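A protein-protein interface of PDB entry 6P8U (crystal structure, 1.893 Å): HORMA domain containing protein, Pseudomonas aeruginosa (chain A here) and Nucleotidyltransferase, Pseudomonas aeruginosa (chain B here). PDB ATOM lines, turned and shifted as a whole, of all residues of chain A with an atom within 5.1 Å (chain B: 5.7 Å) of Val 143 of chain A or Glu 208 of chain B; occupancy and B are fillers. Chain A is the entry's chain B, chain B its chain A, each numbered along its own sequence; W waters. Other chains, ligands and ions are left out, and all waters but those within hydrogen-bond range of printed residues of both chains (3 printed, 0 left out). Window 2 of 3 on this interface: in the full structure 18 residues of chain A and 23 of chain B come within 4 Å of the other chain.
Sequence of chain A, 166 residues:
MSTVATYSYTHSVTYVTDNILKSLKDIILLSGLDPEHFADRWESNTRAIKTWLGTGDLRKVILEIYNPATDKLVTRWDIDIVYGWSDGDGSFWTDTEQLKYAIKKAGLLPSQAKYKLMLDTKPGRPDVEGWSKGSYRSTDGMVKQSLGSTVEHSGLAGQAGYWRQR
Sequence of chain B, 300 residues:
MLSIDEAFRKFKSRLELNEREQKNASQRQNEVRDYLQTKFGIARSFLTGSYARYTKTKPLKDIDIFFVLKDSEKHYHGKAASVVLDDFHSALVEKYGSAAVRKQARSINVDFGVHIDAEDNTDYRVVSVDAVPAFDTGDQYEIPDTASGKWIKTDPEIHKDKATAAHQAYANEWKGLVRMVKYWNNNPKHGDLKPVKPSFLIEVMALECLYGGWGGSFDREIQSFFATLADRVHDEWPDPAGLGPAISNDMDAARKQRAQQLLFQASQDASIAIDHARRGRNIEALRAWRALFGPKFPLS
Among the printed residues, merely in contact across the chains: Arg 164 of chain A with Tyr 211 of chain B (3.3 Å), Gln 145 of chain A with Tyr 211 of chain B (3.3 Å), Val 143 of chain A with Glu 208 of chain B (3.5 Å), Tyr 162 of chain A with Tyr 211 of chain B (3.6 Å), Gln 145 of chain A with Glu 208 of chain B (3.6 Å), Lys 144 of chain A with Arg 232 of chain B (3.9 Å) and Val 143 of chain A with Arg 232 of chain B (3.9 Å).
Of chain B, only Glu 208 (3.5 Å) and Arg 232 (3.9 Å) come within 4 Å of Val 143 of chain A. Glu 208 of chain B touches just these residues of chain A: Val 143, Gln 145 and Arg 164. Of the printed residues of chain B, Tyr 162 of chain A touches Tyr 211. Printed residues of chain A within 4 Å of Tyr 211 of chain B: Gln 145 (3.3 Å), Tyr 162 (3.6 Å) and Arg 164 (3.3 Å). Printed residues of chain A within 4 Å of Arg 232 of chain B: Val 143 and Lys 144. The nearest printed residue of chain B that does not touch Val 143 of chain A is Tyr 211 of chain B (6.5 Å). The nearest printed residue of chain B that does not touch Arg 164 of chain A is Cys 209 of chain B (4.9 Å).
The guanidinium group (NE) of Arg 164 of chain A lies within hydrogen-bond range of the side-chain amide oxygen (OE1) of Gln 145 of chain A, at 2.9 Å. The indole nitrogen (NE1) of Trp 237 of chain B sits at hydrogen-bond distance from the backbone carbonyl oxygen (O) of Arg 232 of chain B. N of Arg 164 of chain A sits at hydrogen-bond distance from O of Val 143 of chain A (2.8 Å). OE2 of Glu 208 of chain B lies within salt-bridge range of NH1 of Arg 232 of chain B. SG of Cys 209 of chain B sits at hydrogen-bond distance from O of Met 205 of chain B. The backbone carbonyl oxygen (O) of Tyr 162 of chain A sits at hydrogen-bond distance from the backbone NH (N) of Gln 145 of chain A.
Water W3 lies within hydrogen-bond range of the backbone carbonyl oxygen (O) of Lys 144 of chain A (2.8 Å), the side-chain amide oxygen (OE1) of Gln 145 of chain A (2.9 Å) and the guanidinium group (NH1) of Arg 232 of chain B (3.0 Å). Water W1 lies within hydrogen-bond range of O of Gln 165 of chain A (2.9 Å) and OH of Tyr 211 of chain B (3.1 Å). Water W2 bridges the backbone carbonyl oxygen (O) of Arg 166 of chain A and the side-chain carboxylate (OE2) of Glu 208 of chain B.
O of Glu 208 of chain B is in hydrogen-bond range of NH2 of Arg 164 of chain A, 2.8 Å away. O of Cys 209 of chain B is in hydrogen-bond range of NE2 of Gln 145 of chain A.
Of the 10 printed residues of chain B, 4 touch a printed residue of chain A. Hydrophobic or aromatic side chains of chain B that line the printed part of chain A: Tyr 211. Of the 10 printed residues of chain A, 5 touch a printed residue of chain B. Hydrophobic or aromatic side chains of chain A within 4 Å of the printed part of chain B: Val 143 and Tyr 162. Along chain A the printed residues that touch a printed residue of chain B span positions 143 to 164. Among the printed residues, no Asp or Glu carboxylate lies within 4 Å of a Lys or Arg side-chain nitrogen of the other chain.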
ATOM      1  N   GLY A 141     -27.686 -32.989  18.687  1.00  0.00           N
ATOM      2  CA  GLY A 141     -26.463 -32.829  17.925  1.00  0.00           C
ATOM      3  C   GLY A 141     -26.651 -32.545  16.453  1.00  0.00           C
ATOM      4  O   GLY A 141     -25.672 -32.585  15.701  1.00  0.00           O
ATOM      5  N   MET A 142     -27.875 -32.260  16.018  1.00  0.00           N
ATOM      6  CA  MET A 142     -28.170 -32.012  14.617  1.00  0.00           C
ATOM      7  C   MET A 142     -28.838 -30.654  14.458  1.00  0.00           C
ATOM      8  O   MET A 142     -29.496 -30.156  15.378  1.00  0.00           O
ATOM      9  CB  MET A 142     -29.076 -33.103  14.032  1.00  0.00           C
ATOM     10  CG  MET A 142     -28.539 -34.518  14.240  1.00  0.00           C
ATOM     11  SD  MET A 142     -29.505 -35.816  13.423  1.00  0.00           S
ATOM     12  CE  MET A 142     -28.839 -35.715  11.761  1.00  0.00           C
ATOM     13  N   VAL A 143     -28.642 -30.054  13.277  1.00  0.00           N
ATOM     14  CA  VAL A 143     -29.314 -28.823  12.891  1.00  0.00           C
ATOM     15  C   VAL A 143     -29.889 -29.029  11.498  1.00  0.00           C
ATOM     16  O   VAL A 143     -29.517 -29.959  10.778  1.00  0.00           O
ATOM     17  CB  VAL A 143     -28.388 -27.590  12.906  1.00  0.00           C
ATOM     18  CG1 VAL A 143     -27.978 -27.256  14.335  1.00  0.00           C
ATOM     19  CG2 VAL A 143     -27.160 -27.821  12.022  1.00  0.00           C
ATOM     20  N   LYS A 144     -30.802 -28.138  11.126  1.00  0.00           N
ATOM     21  CA  LYS A 144     -31.588 -28.257   9.903  1.00  0.00           C
ATOM     22  C   LYS A 144     -31.086 -27.279   8.852  1.00  0.00           C
ATOM     23  O   LYS A 144     -30.844 -26.103   9.148  1.00  0.00           O
ATOM     24  CB  LYS A 144     -33.070 -28.021  10.207  1.00  0.00           C
ATOM     25  CG  LYS A 144     -34.012 -28.083   9.031  1.00  0.00           C
ATOM     26  CD  LYS A 144     -35.411 -27.767   9.527  1.00  0.00           C
ATOM     27  CE  LYS A 144     -36.385 -27.456   8.407  1.00  0.00           C
ATOM     28  NZ  LYS A 144     -37.701 -27.032   8.973  1.00  0.00           N
ATOM     29  N   GLN A 145     -30.919 -27.777   7.633  1.00  0.00           N
ATOM     30  CA  GLN A 145     -30.577 -26.965   6.478  1.00  0.00           C
ATOM     31  C   GLN A 145     -31.820 -26.829   5.607  1.00  0.00           C
ATOM     32  O   GLN A 145     -32.417 -27.831   5.210  1.00  0.00           O
ATOM     33  CB  GLN A 145     -29.429 -27.584   5.674  1.00  0.00           C
ATOM     34  CG  GLN A 145     -28.158 -27.827   6.472  1.00  0.00           C
ATOM     35  CD  GLN A 145     -27.441 -26.543   6.865  1.00  0.00           C
ATOM     36  OE1 GLN A 145     -26.741 -26.505   7.883  1.00  0.00           O
ATOM     37  NE2 GLN A 145     -27.587 -25.504   6.051  1.00  0.00           N
ATOM     38  N   TYR A 162     -33.186 -30.516   5.390  1.00  0.00           N
ATOM     39  CA  TYR A 162     -32.563 -31.751   5.847  1.00  0.00           C
ATOM     40  C   TYR A 162     -31.725 -31.503   7.089  1.00  0.00           C
ATOM     41  O   TYR A 162     -31.061 -30.470   7.213  1.00  0.00           O
ATOM     42  CB  TYR A 162     -31.689 -32.394   4.739  1.00  0.00           C
ATOM     43  CG  TYR A 162     -30.473 -31.596   4.335  1.00  0.00           C
ATOM     44  CD1 TYR A 162     -29.273 -31.722   5.028  1.00  0.00           C
ATOM     45  CD2 TYR A 162     -30.511 -30.733   3.243  1.00  0.00           C
ATOM     46  CE1 TYR A 162     -28.157 -31.005   4.658  1.00  0.00           C
ATOM     47  CE2 TYR A 162     -29.396 -30.005   2.870  1.00  0.00           C
ATOM     48  CZ  TYR A 162     -28.219 -30.147   3.578  1.00  0.00           C
ATOM     49  OH  TYR A 162     -27.108 -29.424   3.199  1.00  0.00           O
ATOM     50  N   TRP A 163     -31.755 -32.463   8.006  1.00  0.00           N
ATOM     51  CA  TRP A 163     -30.984 -32.387   9.239  1.00  0.00           C
ATOM     52  C   TRP A 163     -29.616 -33.019   9.045  1.00  0.00           C
ATOM     53  O   TRP A 163     -29.478 -34.042   8.362  1.00  0.00           O
ATOM     54  CB  TRP A 163     -31.732 -33.086  10.378  1.00  0.00           C
ATOM     55  CG  TRP A 163     -32.972 -32.358  10.800  1.00  0.00           C
ATOM     56  CD1 TRP A 163     -34.187 -32.360  10.166  1.00  0.00           C
ATOM     57  CD2 TRP A 163     -33.118 -31.514  11.942  1.00  0.00           C
ATOM     58  NE1 TRP A 163     -35.074 -31.567  10.843  1.00  0.00           N
ATOM     59  CE2 TRP A 163     -34.447 -31.038  11.942  1.00  0.00           C
ATOM     60  CE3 TRP A 163     -32.258 -31.110  12.963  1.00  0.00           C
ATOM     61  CZ2 TRP A 163     -34.932 -30.180  12.925  1.00  0.00           C
ATOM     62  CZ3 TRP A 163     -32.746 -30.255  13.941  1.00  0.00           C
ATOM     63  CH2 TRP A 163     -34.071 -29.797  13.909  1.00  0.00           C
ATOM     64  N   ARG A 164     -28.605 -32.410   9.663  1.00  0.00           N
ATOM     65  CA  ARG A 164     -27.229 -32.876   9.573  1.00  0.00           C
ATOM     66  C   ARG A 164     -26.554 -32.655  10.915  1.00  0.00           C
ATOM     67  O   ARG A 164     -27.051 -31.913  11.765  1.00  0.00           O
ATOM     68  CB  ARG A 164     -26.471 -32.160   8.442  1.00  0.00           C
ATOM     69  CG  ARG A 164     -26.535 -30.644   8.479  1.00  0.00           C
ATOM     70  CD  ARG A 164     -25.514 -30.074   9.442  1.00  0.00           C
ATOM     71  NE  ARG A 164     -25.389 -28.618   9.336  1.00  0.00           N
ATOM     72  CZ  ARG A 164     -24.476 -27.906   9.991  1.00  0.00           C
ATOM     73  NH1 ARG A 164     -23.609 -28.513  10.794  1.00  0.00           N
ATOM     74  NH2 ARG A 164     -24.423 -26.592   9.835  1.00  0.00           N
ATOM     75  N   GLN A 165     -25.399 -33.293  11.091  1.00  0.00           N
ATOM     76  CA  GLN A 165     -24.705 -33.285  12.368  1.00  0.00           C
ATOM     77  C   GLN A 165     -24.002 -31.952  12.615  1.00  0.00           C
ATOM     78  O   GLN A 165     -23.498 -31.304  11.695  1.00  0.00           O
ATOM     79  CB  GLN A 165     -23.672 -34.410  12.423  1.00  0.00           C
ATOM     80  CG  GLN A 165     -24.226 -35.795  12.117  1.00  0.00           C
ATOM     81  CD  GLN A 165     -24.995 -36.388  13.280  1.00  0.00           C
ATOM     82  OE1 GLN A 165     -24.869 -35.935  14.418  1.00  0.00           O
ATOM     83  NE2 GLN A 165     -25.799 -37.408  12.997  1.00  0.00           N
ATOM     84  N   ARG A 166     -23.965 -31.556  13.884  1.00  0.00           N
ATOM     85  CA  ARG A 166     -23.166 -30.422  14.340  1.00  0.00           C
ATOM     86  C   ARG A 166     -23.926 -29.111  14.203  1.00  0.00           C
ATOM     87  O   ARG A 166     -24.628 -28.702  15.128  1.00  0.00           O
ATOM     88  CB  ARG A 166     -21.840 -30.344  13.565  1.00  0.00           C
ATOM     89  N   VAL B 204     -22.449 -14.321  11.203  1.00  0.00           N
ATOM     90  CA  VAL B 204     -22.376 -15.307  12.278  1.00  0.00           C
ATOM     91  C   VAL B 204     -23.232 -16.523  11.947  1.00  0.00           C
ATOM     92  O   VAL B 204     -22.806 -17.672  12.124  1.00  0.00           O
ATOM     93  CB  VAL B 204     -22.797 -14.674  13.613  1.00  0.00           C
ATOM     94  CG1 VAL B 204     -23.026 -15.741  14.665  1.00  0.00           C
ATOM     95  CG2 VAL B 204     -21.727 -13.684  14.082  1.00  0.00           C
ATOM     96  N   MET B 205     -24.460 -16.288  11.486  1.00  0.00           N
ATOM     97  CA  MET B 205     -25.295 -17.402  11.060  1.00  0.00           C
ATOM     98  C   MET B 205     -24.674 -18.153   9.895  1.00  0.00           C
ATOM     99  O   MET B 205     -24.806 -19.380   9.814  1.00  0.00           O
ATOM    100  CB  MET B 205     -26.690 -16.894  10.676  1.00  0.00           C
ATOM    101  CG  MET B 205     -27.456 -16.258  11.849  1.00  0.00           C
ATOM    102  SD  MET B 205     -29.121 -15.705  11.415  1.00  0.00           S
ATOM    103  CE  MET B 205     -29.883 -17.278  10.989  1.00  0.00           C
ATOM    104  N   ALA B 206     -23.992 -17.442   8.996  1.00  0.00           N
ATOM    105  CA  ALA B 206     -23.366 -18.080   7.845  1.00  0.00           C
ATOM    106  C   ALA B 206     -22.320 -19.101   8.265  1.00  0.00           C
ATOM    107  O   ALA B 206     -22.136 -20.104   7.576  1.00  0.00           O
ATOM    108  CB  ALA B 206     -22.721 -17.021   6.947  1.00  0.00           C
ATOM    109  N   LEU B 207     -21.617 -18.871   9.381  1.00  0.00           N
ATOM    110  CA  LEU B 207     -20.622 -19.839   9.834  1.00  0.00           C
ATOM    111  C   LEU B 207     -21.223 -21.238   9.929  1.00  0.00           C
ATOM    112  O   LEU B 207     -20.530 -22.232   9.687  1.00  0.00           O
ATOM    113  CB  LEU B 207     -20.049 -19.418  11.188  1.00  0.00           C
ATOM    114  CG  LEU B 207     -19.204 -18.146  11.255  1.00  0.00           C
ATOM    115  CD1 LEU B 207     -18.982 -17.721  12.702  1.00  0.00           C
ATOM    116  CD2 LEU B 207     -17.865 -18.322  10.568  1.00  0.00           C
ATOM    117  N   GLU B 208     -22.512 -21.335  10.263  1.00  0.00           N
ATOM    118  CA  GLU B 208     -23.212 -22.606  10.393  1.00  0.00           C
ATOM    119  C   GLU B 208     -24.201 -22.858   9.265  1.00  0.00           C
ATOM    120  O   GLU B 208     -24.328 -23.994   8.804  1.00  0.00           O
ATOM    121  CB  GLU B 208     -23.948 -22.642  11.740  1.00  0.00           C
ATOM    122  CG  GLU B 208     -24.082 -24.016  12.355  1.00  0.00           C
ATOM    123  CD  GLU B 208     -24.640 -23.966  13.772  1.00  0.00           C
ATOM    124  OE1 GLU B 208     -24.027 -23.301  14.638  1.00  0.00           O
ATOM    125  OE2 GLU B 208     -25.703 -24.581  14.011  1.00  0.00           O
ATOM    126  N   CYS B 209     -24.903 -21.821   8.794  1.00  0.00           N
ATOM    127  CA  CYS B 209     -25.963 -22.022   7.808  1.00  0.00           C
ATOM    128  C   CYS B 209     -25.409 -22.347   6.423  1.00  0.00           C
ATOM    129  O   CYS B 209     -26.068 -23.043   5.642  1.00  0.00           O
ATOM    130  CB  CYS B 209     -26.852 -20.781   7.745  1.00  0.00           C
ATOM    131  SG  CYS B 209     -27.758 -20.458   9.278  1.00  0.00           S
ATOM    132  N   LEU B 210     -24.216 -21.853   6.090  1.00  0.00           N
ATOM    133  CA  LEU B 210     -23.521 -22.288   4.880  1.00  0.00           C
ATOM    134  C   LEU B 210     -22.797 -23.587   5.221  1.00  0.00           C
ATOM    135  O   LEU B 210     -21.783 -23.575   5.932  1.00  0.00           O
ATOM    136  CB  LEU B 210     -22.566 -21.206   4.383  1.00  0.00           C
ATOM    137  CG  LEU B 210     -23.246 -19.989   3.737  1.00  0.00           C
ATOM    138  CD1 LEU B 210     -22.241 -18.991   3.207  1.00  0.00           C
ATOM    139  CD2 LEU B 210     -24.187 -20.423   2.608  1.00  0.00           C
ATOM    140  N   TYR B 211     -23.309 -24.706   4.711  1.00  0.00           N
ATOM    141  CA  TYR B 211     -22.899 -26.017   5.170  1.00  0.00           C
ATOM    142  C   TYR B 211     -22.565 -26.928   4.000  1.00  0.00           C
ATOM    143  O   TYR B 211     -23.171 -26.861   2.934  1.00  0.00           O
ATOM    144  CB  TYR B 211     -24.012 -26.702   6.019  1.00  0.00           C
ATOM    145  CG  TYR B 211     -23.763 -28.172   6.242  1.00  0.00           C
ATOM    146  CD1 TYR B 211     -22.873 -28.589   7.218  1.00  0.00           C
ATOM    147  CD2 TYR B 211     -24.401 -29.140   5.481  1.00  0.00           C
ATOM    148  CE1 TYR B 211     -22.625 -29.919   7.435  1.00  0.00           C
ATOM    149  CE2 TYR B 211     -24.164 -30.482   5.695  1.00  0.00           C
ATOM    150  CZ  TYR B 211     -23.277 -30.872   6.673  1.00  0.00           C
ATOM    151  OH  TYR B 211     -23.019 -32.209   6.904  1.00  0.00           O
ATOM    152  N   ARG B 232     -33.868 -19.964  10.749  1.00  0.00           N
ATOM    153  CA  ARG B 232     -33.043 -20.014  11.950  1.00  0.00           C
ATOM    154  C   ARG B 232     -32.760 -18.658  12.584  1.00  0.00           C
ATOM    155  O   ARG B 232     -32.012 -18.593  13.571  1.00  0.00           O
ATOM    156  CB  ARG B 232     -31.706 -20.706  11.639  1.00  0.00           C
ATOM    157  CG  ARG B 232     -31.854 -22.164  11.208  1.00  0.00           C
ATOM    158  CD  ARG B 232     -30.526 -22.905  11.322  1.00  0.00           C
ATOM    159  NE  ARG B 232     -30.090 -22.973  12.711  1.00  0.00           N
ATOM    160  CZ  ARG B 232     -28.874 -23.359  13.102  1.00  0.00           C
ATOM    161  NH1 ARG B 232     -27.959 -23.721  12.204  1.00  0.00           N
ATOM    162  NH2 ARG B 232     -28.579 -23.385  14.393  1.00  0.00           N
ATOM    163  N   TRP B 237     -28.075 -17.054  18.743  1.00  0.00           N
ATOM    164  CA  TRP B 237     -26.806 -16.996  18.019  1.00  0.00           C
ATOM    165  C   TRP B 237     -25.779 -16.306  18.904  1.00  0.00           C
ATOM    166  O   TRP B 237     -25.624 -15.073  18.859  1.00  0.00           O
ATOM    167  CB  TRP B 237     -26.972 -16.272  16.689  1.00  0.00           C
ATOM    168  CG  TRP B 237     -27.721 -17.112  15.714  1.00  0.00           C
ATOM    169  CD1 TRP B 237     -29.056 -17.022  15.391  1.00  0.00           C
ATOM    170  CD2 TRP B 237     -27.200 -18.222  14.973  1.00  0.00           C
ATOM    171  NE1 TRP B 237     -29.381 -17.997  14.474  1.00  0.00           N
ATOM    172  CE2 TRP B 237     -28.262 -18.750  14.206  1.00  0.00           C
ATOM    173  CE3 TRP B 237     -25.941 -18.813  14.877  1.00  0.00           C
ATOM    174  CZ2 TRP B 237     -28.090 -19.815  13.339  1.00  0.00           C
ATOM    175  CZ3 TRP B 237     -25.783 -19.889  14.028  1.00  0.00           C
ATOM    176  CH2 TRP B 237     -26.849 -20.380  13.276  1.00  0.00           C
HETATM  177  O   HOH W   1     -21.779 -32.531   9.770  1.00  0.00           O
HETATM  178  O   HOH W   2     -24.598 -26.255  16.750  1.00  0.00           O
HETATM  179  O   HOH W   3     -28.403 -24.839   9.491  1.00  0.00           O
